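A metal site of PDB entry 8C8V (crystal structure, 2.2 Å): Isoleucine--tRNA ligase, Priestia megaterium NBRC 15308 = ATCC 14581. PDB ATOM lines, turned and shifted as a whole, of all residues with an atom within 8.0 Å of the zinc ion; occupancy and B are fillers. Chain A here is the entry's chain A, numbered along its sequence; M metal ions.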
ATOM      1  N   GLU A 458       8.063  -1.020  10.197  1.00  0.00           N
ATOM      2  CA  GLU A 458       7.914   0.269  10.844  1.00  0.00           C
ATOM      3  C   GLU A 458       8.706   1.320  10.099  1.00  0.00           C
ATOM      4  O   GLU A 458       9.858   1.096   9.719  1.00  0.00           O
ATOM      5  CB  GLU A 458       8.379   0.230  12.301  1.00  0.00           C
ATOM      6  CG  GLU A 458       7.786  -0.885  13.131  1.00  0.00           C
ATOM      7  CD  GLU A 458       8.408  -0.937  14.504  1.00  0.00           C
ATOM      8  OE1 GLU A 458       8.040  -0.094  15.352  1.00  0.00           O
ATOM      9  OE2 GLU A 458       9.284  -1.808  14.734  1.00  0.00           O
ATOM     10  N   CYS A 459       8.088   2.481   9.902  1.00  0.00           N
ATOM     11  CA  CYS A 459       8.747   3.581   9.234  1.00  0.00           C
ATOM     12  C   CYS A 459       9.835   4.165  10.130  1.00  0.00           C
ATOM     13  O   CYS A 459       9.571   4.560  11.272  1.00  0.00           O
ATOM     14  CB  CYS A 459       7.733   4.650   8.852  1.00  0.00           C
ATOM     15  SG  CYS A 459       8.495   6.101   8.102  1.00  0.00           S
ATOM     16  N   GLU A 460      11.061   4.243   9.605  1.00  0.00           N
ATOM     17  CA  GLU A 460      12.157   4.883  10.331  1.00  0.00           C
ATOM     18  C   GLU A 460      11.833   6.329  10.654  1.00  0.00           C
ATOM     19  O   GLU A 460      12.291   6.855  11.673  1.00  0.00           O
ATOM     20  CB  GLU A 460      13.444   4.804   9.510  1.00  0.00           C
ATOM     21  CG  GLU A 460      13.986   3.402   9.330  1.00  0.00           C
ATOM     22  CD  GLU A 460      14.782   2.929  10.532  1.00  0.00           C
ATOM     23  OE1 GLU A 460      15.884   3.462  10.767  1.00  0.00           O
ATOM     24  OE2 GLU A 460      14.294   2.039  11.257  1.00  0.00           O
ATOM     25  N   GLY A 461      11.054   6.998   9.803  1.00  0.00           N
ATOM     26  CA  GLY A 461      10.752   8.394   9.998  1.00  0.00           C
ATOM     27  C   GLY A 461       9.661   8.681  11.010  1.00  0.00           C
ATOM     28  O   GLY A 461       9.894   9.403  11.982  1.00  0.00           O
ATOM     29  N   CYS A 462       8.474   8.111  10.796  1.00  0.00           N
ATOM     30  CA  CYS A 462       7.296   8.456  11.593  1.00  0.00           C
ATOM     31  C   CYS A 462       6.711   7.288  12.374  1.00  0.00           C
ATOM     32  O   CYS A 462       5.651   7.460  12.987  1.00  0.00           O
ATOM     33  CB  CYS A 462       6.205   9.046  10.695  1.00  0.00           C
ATOM     34  SG  CYS A 462       5.402   7.807   9.691  1.00  0.00           S
ATOM     35  N   GLN A 463       7.334   6.104  12.342  1.00  0.00           N
ATOM     36  CA  GLN A 463       6.974   4.929  13.130  1.00  0.00           C
ATOM     37  C   GLN A 463       5.636   4.320  12.746  1.00  0.00           C
ATOM     38  O   GLN A 463       5.125   3.448  13.459  1.00  0.00           O
ATOM     39  CB  GLN A 463       6.997   5.210  14.643  1.00  0.00           C
ATOM     40  CG  GLN A 463       8.398   5.349  15.229  1.00  0.00           C
ATOM     41  CD  GLN A 463       9.143   6.543  14.673  1.00  0.00           C
ATOM     42  OE1 GLN A 463       8.749   7.689  14.894  1.00  0.00           O
ATOM     43  NE2 GLN A 463      10.214   6.283  13.925  1.00  0.00           N
ATOM     44  N   HIS A 464       5.046   4.749  11.620  1.00  0.00           N
ATOM     45  CA  HIS A 464       3.869   4.081  11.081  1.00  0.00           C
ATOM     46  C   HIS A 464       4.174   2.612  10.823  1.00  0.00           C
ATOM     47  O   HIS A 464       5.293   2.236  10.477  1.00  0.00           O
ATOM     48  CB  HIS A 464       3.433   4.776   9.793  1.00  0.00           C
ATOM     49  CG  HIS A 464       2.255   4.148   9.124  1.00  0.00           C
ATOM     50  ND1 HIS A 464       0.974   4.225   9.643  1.00  0.00           N
ATOM     51  CD2 HIS A 464       2.154   3.447   7.966  1.00  0.00           C
ATOM     52  CE1 HIS A 464       0.145   3.579   8.840  1.00  0.00           C
ATOM     53  NE2 HIS A 464       0.830   3.100   7.817  1.00  0.00           N
ATOM     54  N   GLN A 465       3.155   1.766  11.025  1.00  0.00           N
ATOM     55  CA  GLN A 465       3.326   0.324  10.916  1.00  0.00           C
ATOM     56  C   GLN A 465       2.512  -0.225   9.746  1.00  0.00           C
ATOM     57  O   GLN A 465       1.378   0.208   9.508  1.00  0.00           O
ATOM     58  CB  GLN A 465       2.896  -0.375  12.210  1.00  0.00           C
ATOM     59  CG  GLN A 465       3.681   0.055  13.425  1.00  0.00           C
ATOM     60  CD  GLN A 465       3.199  -0.612  14.698  1.00  0.00           C
ATOM     61  OE1 GLN A 465       2.267  -1.430  14.669  1.00  0.00           O
ATOM     62  NE2 GLN A 465       3.814  -0.271  15.818  1.00  0.00           N
ATOM     63  N   THR A 499       8.005   1.417   1.361  1.00  0.00           N
ATOM     64  CA  THR A 499       7.846   2.868   1.336  1.00  0.00           C
ATOM     65  C   THR A 499       6.673   3.230   2.234  1.00  0.00           C
ATOM     66  O   THR A 499       5.587   2.654   2.096  1.00  0.00           O
ATOM     67  CB  THR A 499       7.623   3.375  -0.087  1.00  0.00           C
ATOM     68  OG1 THR A 499       8.727   2.983  -0.918  1.00  0.00           O
ATOM     69  CG2 THR A 499       7.498   4.887  -0.107  1.00  0.00           C
ATOM     70  N   CYS A 500       6.894   4.168   3.139  1.00  0.00           N
ATOM     71  CA  CYS A 500       5.848   4.533   4.095  1.00  0.00           C
ATOM     72  C   CYS A 500       4.709   5.250   3.381  1.00  0.00           C
ATOM     73  O   CYS A 500       4.953   6.259   2.693  1.00  0.00           O
ATOM     74  CB  CYS A 500       6.414   5.407   5.204  1.00  0.00           C
ATOM     75  SG  CYS A 500       5.159   6.065   6.346  1.00  0.00           S
ATOM     76  N   PRO A 501       3.465   4.791   3.508  1.00  0.00           N
ATOM     77  CA  PRO A 501       2.346   5.511   2.896  1.00  0.00           C
ATOM     78  C   PRO A 501       2.118   6.898   3.475  1.00  0.00           C
ATOM     79  O   PRO A 501       1.421   7.713   2.848  1.00  0.00           O
ATOM     80  CB  PRO A 501       1.144   4.595   3.150  1.00  0.00           C
ATOM     81  CG  PRO A 501       1.542   3.768   4.327  1.00  0.00           C
ATOM     82  CD  PRO A 501       3.019   3.564   4.203  1.00  0.00           C
ATOM     83  N   VAL A 502       2.675   7.203   4.640  1.00  0.00           N
ATOM     84  CA  VAL A 502       2.428   8.472   5.314  1.00  0.00           C
ATOM     85  C   VAL A 502       3.462   9.515   4.895  1.00  0.00           C
ATOM     86  O   VAL A 502       3.101  10.595   4.411  1.00  0.00           O
ATOM     87  CB  VAL A 502       2.420   8.298   6.841  1.00  0.00           C
ATOM     88  CG1 VAL A 502       2.370   9.658   7.530  1.00  0.00           C
ATOM     89  CG2 VAL A 502       1.241   7.436   7.266  1.00  0.00           C
ATOM     90  N   CYS A 503       4.741   9.215   5.090  1.00  0.00           N
ATOM     91  CA  CYS A 503       5.798  10.189   4.849  1.00  0.00           C
ATOM     92  C   CYS A 503       6.779   9.775   3.763  1.00  0.00           C
ATOM     93  O   CYS A 503       7.728  10.520   3.500  1.00  0.00           O
ATOM     94  CB  CYS A 503       6.571  10.452   6.142  1.00  0.00           C
ATOM     95  SG  CYS A 503       7.660   9.108   6.640  1.00  0.00           S
ATOM     96  N   SER A 504       6.582   8.616   3.138  1.00  0.00           N
ATOM     97  CA  SER A 504       7.471   8.067   2.114  1.00  0.00           C
ATOM     98  C   SER A 504       8.857   7.716   2.657  1.00  0.00           C
ATOM     99  O   SER A 504       9.789   7.527   1.873  1.00  0.00           O
ATOM    100  CB  SER A 504       7.597   9.015   0.914  1.00  0.00           C
ATOM    101  OG  SER A 504       7.685   8.291  -0.309  1.00  0.00           O
ATOM    102  N   GLY A 505       9.009   7.627   3.972  1.00  0.00           N
ATOM    103  CA  GLY A 505      10.265   7.185   4.551  1.00  0.00           C
ATOM    104  C   GLY A 505      10.453   5.686   4.403  1.00  0.00           C
ATOM    105  O   GLY A 505       9.571   4.950   3.962  1.00  0.00           O
ATOM    106  N   GLU A 506      11.641   5.226   4.788  1.00  0.00           N
ATOM    107  CA  GLU A 506      11.976   3.804   4.701  1.00  0.00           C
ATOM    108  C   GLU A 506      11.322   3.025   5.833  1.00  0.00           C
ATOM    109  O   GLU A 506      11.424   3.412   7.006  1.00  0.00           O
ATOM    110  CB  GLU A 506      13.492   3.614   4.735  1.00  0.00           C
ATOM    111  CG  GLU A 506      13.940   2.165   4.568  1.00  0.00           C
ATOM    112  CD  GLU A 506      15.431   1.976   4.811  1.00  0.00           C
ATOM    113  OE1 GLU A 506      16.010   2.717   5.627  1.00  0.00           O
ATOM    114  OE2 GLU A 506      16.017   1.074   4.181  1.00  0.00           O
ATOM    115  N   MET A 507      10.657   1.926   5.493  1.00  0.00           N
ATOM    116  CA  MET A 507      10.082   1.027   6.486  1.00  0.00           C
ATOM    117  C   MET A 507      10.951  -0.212   6.590  1.00  0.00           C
ATOM    118  O   MET A 507      11.252  -0.846   5.581  1.00  0.00           O
ATOM    119  CB  MET A 507       8.644   0.633   6.140  1.00  0.00           C
ATOM    120  CG  MET A 507       7.719   1.804   5.803  1.00  0.00           C
ATOM    121  SD  MET A 507       5.981   1.289   5.786  1.00  0.00           S
ATOM    122  CE  MET A 507       5.598   1.309   7.535  1.00  0.00           C
HETATM  123 ZN    ZN M   1       6.554   7.341   7.715  1.00  0.00          ZN
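SG of Cys 462 is bound to the zinc ion, at 2.3 Å.
SG of Cys 500 binds the zinc ion, 2.3 Å away.
SG of Cys 459 is bound to the zinc ion, 2.3 Å away.
SG of Cys 503 is bound to the zinc ion (2.3 Å).
Along chain A the residues within 4 Å of the zinc ion span positions 459 to 503.
SG of Cys 462 lies close to N of His 464 (3.6 Å).
SG of Cys 500 sits close to N of Val 502 (3.2 Å).
N of Cys 500 sits at hydrogen-bond distance from O of Gly 505, at 2.9 Å.
The backbone carbonyl oxygen of His 464 is in hydrogen-bond range of the backbone NH of Cys 459 (2.9 Å).
The backbone NH (N) of Gly 461 sits close to the side-chain sulfur (SG) of Cys 459 (3.2 Å).
The side-chain amide nitrogen (NE2) of Gln 463 sits close to the backbone carbonyl oxygen (O) of Cys 459 (3.2 Å).
The backbone NH (N) of Gly 505 sits close to the side-chain sulfur (SG) of Cys 503.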
